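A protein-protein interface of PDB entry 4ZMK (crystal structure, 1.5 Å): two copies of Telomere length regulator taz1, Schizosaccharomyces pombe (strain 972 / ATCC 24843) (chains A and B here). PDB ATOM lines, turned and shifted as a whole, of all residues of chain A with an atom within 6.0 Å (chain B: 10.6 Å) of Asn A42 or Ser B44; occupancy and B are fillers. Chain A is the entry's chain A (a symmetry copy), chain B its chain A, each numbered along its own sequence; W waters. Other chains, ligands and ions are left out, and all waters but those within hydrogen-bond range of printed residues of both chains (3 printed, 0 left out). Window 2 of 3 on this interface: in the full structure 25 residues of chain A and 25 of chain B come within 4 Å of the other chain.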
ATOM      1  N   LEU A  38      18.546   5.152 -13.320  1.00  0.00           N
ATOM      2  CA  LEU A  38      18.117   3.807 -12.954  1.00  0.00           C
ATOM      3  C   LEU A  38      18.793   2.701 -13.761  1.00  0.00           C
ATOM      4  O   LEU A  38      18.554   1.525 -13.519  1.00  0.00           O
ATOM      5  CB  LEU A  38      16.603   3.693 -13.107  1.00  0.00           C
ATOM      6  CG  LEU A  38      15.866   4.716 -12.265  1.00  0.00           C
ATOM      7  CD1 LEU A  38      14.375   4.635 -12.520  1.00  0.00           C
ATOM      8  CD2 LEU A  38      16.200   4.478 -10.802  1.00  0.00           C
ATOM      9  N   ALA A  40      22.245   2.743 -14.375  1.00  0.00           N
ATOM     10  CA  ALA A  40      23.617   2.636 -13.905  1.00  0.00           C
ATOM     11  C   ALA A  40      23.735   1.656 -12.743  1.00  0.00           C
ATOM     12  O   ALA A  40      24.437   0.651 -12.833  1.00  0.00           O
ATOM     13  CB  ALA A  40      24.140   4.007 -13.493  1.00  0.00           C
ATOM     14  N   ASP A  41      23.036   1.954 -11.656  1.00  0.00           N
ATOM     15  CA  ASP A  41      23.182   1.203 -10.417  1.00  0.00           C
ATOM     16  C   ASP A  41      21.949   1.355  -9.536  1.00  0.00           C
ATOM     17  O   ASP A  41      21.068   2.175  -9.821  1.00  0.00           O
ATOM     18  CB  ASP A  41      24.417   1.675  -9.657  1.00  0.00           C
ATOM     19  CG  ASP A  41      24.323   3.132  -9.250  1.00  0.00           C
ATOM     20  OD1 ASP A  41      23.893   3.409  -8.114  1.00  0.00           O
ATOM     21  OD2 ASP A  41      24.675   4.004 -10.070  1.00  0.00           O
ATOM     22  N   ASN A  42      21.890   0.567  -8.464  1.00  0.00           N
ATOM     23  CA  ASN A  42      20.754   0.621  -7.555  1.00  0.00           C
ATOM     24  C   ASN A  42      21.156   1.024  -6.146  1.00  0.00           C
ATOM     25  O   ASN A  42      20.497   0.650  -5.177  1.00  0.00           O
ATOM     26  CB  ASN A  42      20.010  -0.721  -7.525  1.00  0.00           C
ATOM     27  CG  ASN A  42      20.810  -1.849  -8.132  1.00  0.00           C
ATOM     28  OD1 ASN A  42      21.599  -2.499  -7.442  1.00  0.00           O
ATOM     29  ND2 ASN A  42      20.603  -2.101  -9.428  1.00  0.00           N
ATOM     30  N   LEU A  43      22.241   1.787  -6.042  1.00  0.00           N
ATOM     31  CA  LEU A  43      22.593   2.435  -4.784  1.00  0.00           C
ATOM     32  C   LEU A  43      21.454   3.300  -4.305  1.00  0.00           C
ATOM     33  O   LEU A  43      20.723   3.887  -5.103  1.00  0.00           O
ATOM     34  CB  LEU A  43      23.837   3.294  -4.931  1.00  0.00           C
ATOM     35  CG  LEU A  43      25.136   2.531  -5.134  1.00  0.00           C
ATOM     36  CD1 LEU A  43      26.264   3.511  -5.404  1.00  0.00           C
ATOM     37  CD2 LEU A  43      25.422   1.686  -3.908  1.00  0.00           C
ATOM     38  N   SER A  44      21.307   3.367  -2.994  1.00  0.00           N
ATOM     39  CA  SER A  44      20.259   4.146  -2.384  1.00  0.00           C
ATOM     40  C   SER A  44      20.287   5.603  -2.865  1.00  0.00           C
ATOM     41  O   SER A  44      19.248   6.165  -3.199  1.00  0.00           O
ATOM     42  CB  SER A  44      20.392   4.068  -0.867  1.00  0.00           C
ATOM     43  OG  SER A  44      19.380   4.820  -0.230  1.00  0.00           O
ATOM     44  N   THR A  46      21.541   6.947  -5.610  1.00  0.00           N
ATOM     45  CA  THR A  46      21.113   7.013  -6.991  1.00  0.00           C
ATOM     46  C   THR A  46      19.602   6.885  -7.082  1.00  0.00           C
ATOM     47  O   THR A  46      18.960   7.609  -7.817  1.00  0.00           O
ATOM     48  CB  THR A  46      21.783   5.909  -7.815  1.00  0.00           C
ATOM     49  OG1 THR A  46      23.198   6.140  -7.849  1.00  0.00           O
ATOM     50  CG2 THR A  46      21.231   5.875  -9.230  1.00  0.00           C
ATOM     51  N   VAL A  47      19.039   5.967  -6.311  1.00  0.00           N
ATOM     52  CA  VAL A  47      17.613   5.705  -6.368  1.00  0.00           C
ATOM     53  C   VAL A  47      16.851   6.882  -5.801  1.00  0.00           C
ATOM     54  O   VAL A  47      15.791   7.240  -6.297  1.00  0.00           O
ATOM     55  CB  VAL A  47      17.241   4.426  -5.603  1.00  0.00           C
ATOM     56  CG1 VAL A  47      15.735   4.342  -5.384  1.00  0.00           C
ATOM     57  CG2 VAL A  47      17.743   3.208  -6.357  1.00  0.00           C
ATOM     58  N   LEU B  37       7.433   3.239  -6.476  1.00  0.00           N
ATOM     59  CA  LEU B  37       8.387   2.148  -6.574  1.00  0.00           C
ATOM     60  C   LEU B  37       9.711   2.546  -5.932  1.00  0.00           C
ATOM     61  O   LEU B  37      10.247   1.821  -5.099  1.00  0.00           O
ATOM     62  CB  LEU B  37       8.600   1.731  -8.026  1.00  0.00           C
ATOM     63  CG  LEU B  37       7.482   0.895  -8.640  1.00  0.00           C
ATOM     64  CD1 LEU B  37       7.949   0.244  -9.930  1.00  0.00           C
ATOM     65  CD2 LEU B  37       7.024  -0.161  -7.669  1.00  0.00           C
ATOM     66  N   LEU B  38      10.200   3.728  -6.283  1.00  0.00           N
ATOM     67  CA  LEU B  38      11.491   4.206  -5.801  1.00  0.00           C
ATOM     68  C   LEU B  38      11.484   4.638  -4.337  1.00  0.00           C
ATOM     69  O   LEU B  38      12.517   5.016  -3.799  1.00  0.00           O
ATOM     70  CB  LEU B  38      11.964   5.367  -6.671  1.00  0.00           C
ATOM     71  CG  LEU B  38      12.071   4.979  -8.133  1.00  0.00           C
ATOM     72  CD1 LEU B  38      12.446   6.182  -8.973  1.00  0.00           C
ATOM     73  CD2 LEU B  38      13.087   3.858  -8.269  1.00  0.00           C
ATOM     74  N   ALA B  40       9.916   2.700  -1.871  1.00  0.00           N
ATOM     75  CA  ALA B  40       9.849   1.494  -1.060  1.00  0.00           C
ATOM     76  C   ALA B  40      11.239   0.957  -0.740  1.00  0.00           C
ATOM     77  O   ALA B  40      11.628   0.863   0.421  1.00  0.00           O
ATOM     78  CB  ALA B  40       9.022   0.429  -1.771  1.00  0.00           C
ATOM     79  N   ASP B  41      11.984   0.612  -1.782  1.00  0.00           N
ATOM     80  CA  ASP B  41      13.261  -0.069  -1.623  1.00  0.00           C
ATOM     81  C   ASP B  41      14.145   0.130  -2.848  1.00  0.00           C
ATOM     82  O   ASP B  41      13.692   0.653  -3.873  1.00  0.00           O
ATOM     83  CB  ASP B  41      13.038  -1.560  -1.389  1.00  0.00           C
ATOM     84  CG  ASP B  41      12.353  -2.233  -2.562  1.00  0.00           C
ATOM     85  OD1 ASP B  41      13.056  -2.785  -3.428  1.00  0.00           O
ATOM     86  OD2 ASP B  41      11.107  -2.205  -2.620  1.00  0.00           O
ATOM     87  N   ASN B  42      15.404  -0.289  -2.740  1.00  0.00           N
ATOM     88  CA  ASN B  42      16.341  -0.143  -3.845  1.00  0.00           C
ATOM     89  C   ASN B  42      16.865  -1.479  -4.343  1.00  0.00           C
ATOM     90  O   ASN B  42      17.974  -1.558  -4.871  1.00  0.00           O
ATOM     91  CB  ASN B  42      17.512   0.769  -3.456  1.00  0.00           C
ATOM     92  CG  ASN B  42      17.611   0.992  -1.965  1.00  0.00           C
ATOM     93  OD1 ASN B  42      18.246   0.208  -1.255  1.00  0.00           O
ATOM     94  ND2 ASN B  42      16.994   2.073  -1.478  1.00  0.00           N
ATOM     95  N   LEU B  43      16.062  -2.526  -4.171  1.00  0.00           N
ATOM     96  CA  LEU B  43      16.338  -3.806  -4.811  1.00  0.00           C
ATOM     97  C   LEU B  43      16.444  -3.630  -6.306  1.00  0.00           C
ATOM     98  O   LEU B  43      15.761  -2.794  -6.897  1.00  0.00           O
ATOM     99  CB  LEU B  43      15.253  -4.824  -4.509  1.00  0.00           C
ATOM    100  CG  LEU B  43      15.207  -5.323  -3.074  1.00  0.00           C
ATOM    101  CD1 LEU B  43      13.996  -6.219  -2.886  1.00  0.00           C
ATOM    102  CD2 LEU B  43      16.493  -6.060  -2.755  1.00  0.00           C
ATOM    103  N   SER B  44      17.312  -4.423  -6.908  1.00  0.00           N
ATOM    104  CA  SER B  44      17.532  -4.369  -8.331  1.00  0.00           C
ATOM    105  C   SER B  44      16.221  -4.535  -9.112  1.00  0.00           C
ATOM    106  O   SER B  44      15.962  -3.790 -10.053  1.00  0.00           O
ATOM    107  CB  SER B  44      18.542  -5.442  -8.726  1.00  0.00           C
ATOM    108  OG  SER B  44      18.787  -5.421 -10.116  1.00  0.00           O
ATOM    109  N   GLU B  45      15.388  -5.492  -8.705  1.00  0.00           N
ATOM    110  CA  GLU B  45      14.146  -5.787  -9.418  1.00  0.00           C
ATOM    111  C   GLU B  45      13.189  -4.613  -9.372  1.00  0.00           C
ATOM    112  O   GLU B  45      12.538  -4.298 -10.359  1.00  0.00           O
ATOM    113  CB  GLU B  45      13.446  -7.024  -8.850  1.00  0.00           C
ATOM    114  CG  GLU B  45      14.096  -8.338  -9.223  1.00  0.00           C
ATOM    115  CD  GLU B  45      15.189  -8.749  -8.241  1.00  0.00           C
ATOM    116  OE1 GLU B  45      15.368  -8.047  -7.215  1.00  0.00           O
ATOM    117  OE2 GLU B  45      15.865  -9.777  -8.491  1.00  0.00           O
ATOM    118  N   THR B  46      13.089  -3.989  -8.211  1.00  0.00           N
ATOM    119  CA  THR B  46      12.275  -2.804  -8.051  1.00  0.00           C
ATOM    120  C   THR B  46      12.797  -1.682  -8.931  1.00  0.00           C
ATOM    121  O   THR B  46      12.034  -0.990  -9.577  1.00  0.00           O
ATOM    122  CB  THR B  46      12.257  -2.356  -6.586  1.00  0.00           C
ATOM    123  OG1 THR B  46      11.613  -3.364  -5.794  1.00  0.00           O
ATOM    124  CG2 THR B  46      11.527  -1.033  -6.430  1.00  0.00           C
ATOM    125  N   VAL B  47      14.111  -1.520  -8.965  1.00  0.00           N
ATOM    126  CA  VAL B  47      14.719  -0.435  -9.711  1.00  0.00           C
ATOM    127  C   VAL B  47      14.548  -0.672 -11.194  1.00  0.00           C
ATOM    128  O   VAL B  47      14.327   0.260 -11.957  1.00  0.00           O
ATOM    129  CB  VAL B  47      16.210  -0.281  -9.376  1.00  0.00           C
ATOM    130  CG1 VAL B  47      16.906   0.618 -10.391  1.00  0.00           C
ATOM    131  CG2 VAL B  47      16.372   0.269  -7.971  1.00  0.00           C
ATOM    132  N   SER B  48      14.630  -1.932 -11.598  1.00  0.00           N
ATOM    133  CA  SER B  48      14.497  -2.293 -13.006  1.00  0.00           C
ATOM    134  C   SER B  48      13.059  -2.097 -13.507  1.00  0.00           C
ATOM    135  O   SER B  48      12.839  -1.765 -14.671  1.00  0.00           O
ATOM    136  CB  SER B  48      14.949  -3.739 -13.223  1.00  0.00           C
ATOM    137  OG  SER B  48      14.759  -4.146 -14.566  1.00  0.00           O
ATOM    138  N   GLN B  49      12.084  -2.287 -12.627  1.00  0.00           N
ATOM    139  CA  GLN B  49      10.697  -2.125 -13.014  1.00  0.00           C
ATOM    140  C   GLN B  49      10.393  -0.639 -13.192  1.00  0.00           C
ATOM    141  O   GLN B  49       9.712  -0.251 -14.138  1.00  0.00           O
ATOM    142  CB  GLN B  49       9.766  -2.760 -11.985  1.00  0.00           C
ATOM    143  CG  GLN B  49       8.312  -2.821 -12.421  1.00  0.00           C
ATOM    144  CD  GLN B  49       8.126  -3.569 -13.732  1.00  0.00           C
ATOM    145  OE1 GLN B  49       8.273  -4.786 -13.791  1.00  0.00           O
ATOM    146  NE2 GLN B  49       7.806  -2.837 -14.789  1.00  0.00           N
ATOM    147  N   ALA B  50      10.913   0.181 -12.281  1.00  0.00           N
ATOM    148  CA  ALA B  50      10.782   1.639 -12.353  1.00  0.00           C
ATOM    149  C   ALA B  50      11.432   2.190 -13.627  1.00  0.00           C
ATOM    150  O   ALA B  50      10.903   3.111 -14.257  1.00  0.00           O
ATOM    151  CB  ALA B  50      11.394   2.292 -11.109  1.00  0.00           C
ATOM    152  N   ARG B  51      12.580   1.620 -13.996  1.00  0.00           N
ATOM    153  CA  ARG B  51      13.253   1.980 -15.235  1.00  0.00           C
ATOM    154  C   ARG B  51      12.417   1.594 -16.462  1.00  0.00           C
ATOM    155  O   ARG B  51      12.375   2.333 -17.439  1.00  0.00           O
ATOM    156  CB  ARG B  51      14.627   1.320 -15.300  1.00  0.00           C
ATOM    157  CG  ARG B  51      15.388   1.618 -16.569  1.00  0.00           C
ATOM    158  CD  ARG B  51      16.578   0.683 -16.728  1.00  0.00           C
ATOM    159  NE  ARG B  51      16.232  -0.702 -16.415  1.00  0.00           N
ATOM    160  CZ  ARG B  51      15.533  -1.494 -17.218  1.00  0.00           C
ATOM    161  NH1 ARG B  51      15.104  -1.036 -18.388  1.00  0.00           N
ATOM    162  NH2 ARG B  51      15.261  -2.740 -16.853  1.00  0.00           N
ATOM    163  N   ASP B  52      11.749   0.442 -16.414  1.00  0.00           N
ATOM    164  CA  ASP B  52      10.842   0.066 -17.498  1.00  0.00           C
ATOM    165  C   ASP B  52       9.682   1.047 -17.588  1.00  0.00           C
ATOM    166  O   ASP B  52       9.293   1.453 -18.678  1.00  0.00           O
ATOM    167  CB  ASP B  52      10.291  -1.357 -17.315  1.00  0.00           C
ATOM    168  CG  ASP B  52      11.337  -2.431 -17.576  1.00  0.00           C
ATOM    169  OD1 ASP B  52      12.445  -2.101 -18.048  1.00  0.00           O
ATOM    170  OD2 ASP B  52      11.051  -3.617 -17.320  1.00  0.00           O
HETATM  171  O   HOH W   1      18.717  -2.591 -11.607  1.00  0.00           O
HETATM  172  O   HOH W   2      17.738  -1.341 -13.976  1.00  0.00           O
HETATM  173  O   HOH W   3      16.506   4.952  -1.631  1.00  0.00           O
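The backbone carbonyl oxygen (O) of Asn A42 lies close to the backbone carbonyl oxygen (O) of Asn B42, at 3.4 Å.
Leu A38 touches Val B47, and with the chains exchanged Val A47 touches Leu B38. Asn B42 touches its own counterpart, Asn A42. Asn A42 touches Val B47, and with the chains exchanged Val A47 touches Asn B42. Val A47 touches its own counterpart, Val B47. Positions printed for both chains: 38, 40, 41, 42, 43, 44, 46 and 47. Of the 10 pairs that touch across the chains among the printed residues, 8 have their exchanged pair printed and touching as well.
Of the 8 printed residues of chain A, 4 touch a printed residue of chain B. Along chain A the printed residues that touch a printed residue of chain B span positions 38 to 47. Of the 15 printed residues of chain B, 6 touch a printed residue of chain A. Printed residues of chain B that touch a printed residue of chain A: Leu B38, Asn B42, Ser B44, Val B47, Ala B50 and Arg B51. Hydrophobic or aromatic side chains of chain B within 4 Å of the printed part of chain A: Leu B38 and Val B47. Among the printed residues, no Asp or Glu carboxylate lies within 4 Å of a Lys or Arg side-chain nitrogen of the other chain.
Asp A41 touches none of the printed residues of chain B. Of the printed residues of chain B, Asn A42 touches Asn B42 (3.4 Å), Ser B44 (3.8 Å) and Val B47 (3.8 Å). No residue of chain B comes within 4 Å of Leu A43. Printed residues of chain B within 4 Å of Val A47: Leu B38, Asn B42 and Val B47. Ser B44 touches one residue of chain A. Of the printed residues of chain A, Val B47 touches Leu A38 (3.7 Å), Asn A42 (3.8 Å) and Val A47 (3.6 Å). The nearest residue of chain B that does not touch Asn A42 is Leu B43 (4.8 Å). The nearest printed residue of chain A that does not touch Ser B44 is Leu A38 (6.9 Å).
Water W1 lies within hydrogen-bond range of ND2 of Asn A42 (2.9 Å) and OG of Ser B44 (3.2 Å). Water W3 bridges ND2 of Asn B42 (2.9 Å) and OG of Ser A44 (3.2 Å). Water W2 bridges NE of Arg B51 (2.9 Å) and O of Leu A38 (3.0 Å).
NH2 of Arg B51 sits at hydrogen-bond distance from OG of Ser B48. The guanidinium group (NH1) of Arg B51 is in salt-bridge range of the side-chain carboxylate (OD1) of Asp B52 (2.9 Å).
Leu A38 touches Val B47. CD1 of Leu A38 touches C of Ala B50 (3.98 Å). Leu A38 touches Arg B51 (CB to CB, 3.8 Å). OG of Ser B44 touches ND2 of Asn A42 (3.8 Å). Asn A42 touches Val B47. Ser A44 touches Asn B42 (OG to ND2, 3.8 Å). Val A47 touches Leu B38 (CG1 to O, 3.6 Å). Asn B42 touches Val A47 (CB to CG2, 3.8 Å). Val B47 touches Val A47.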
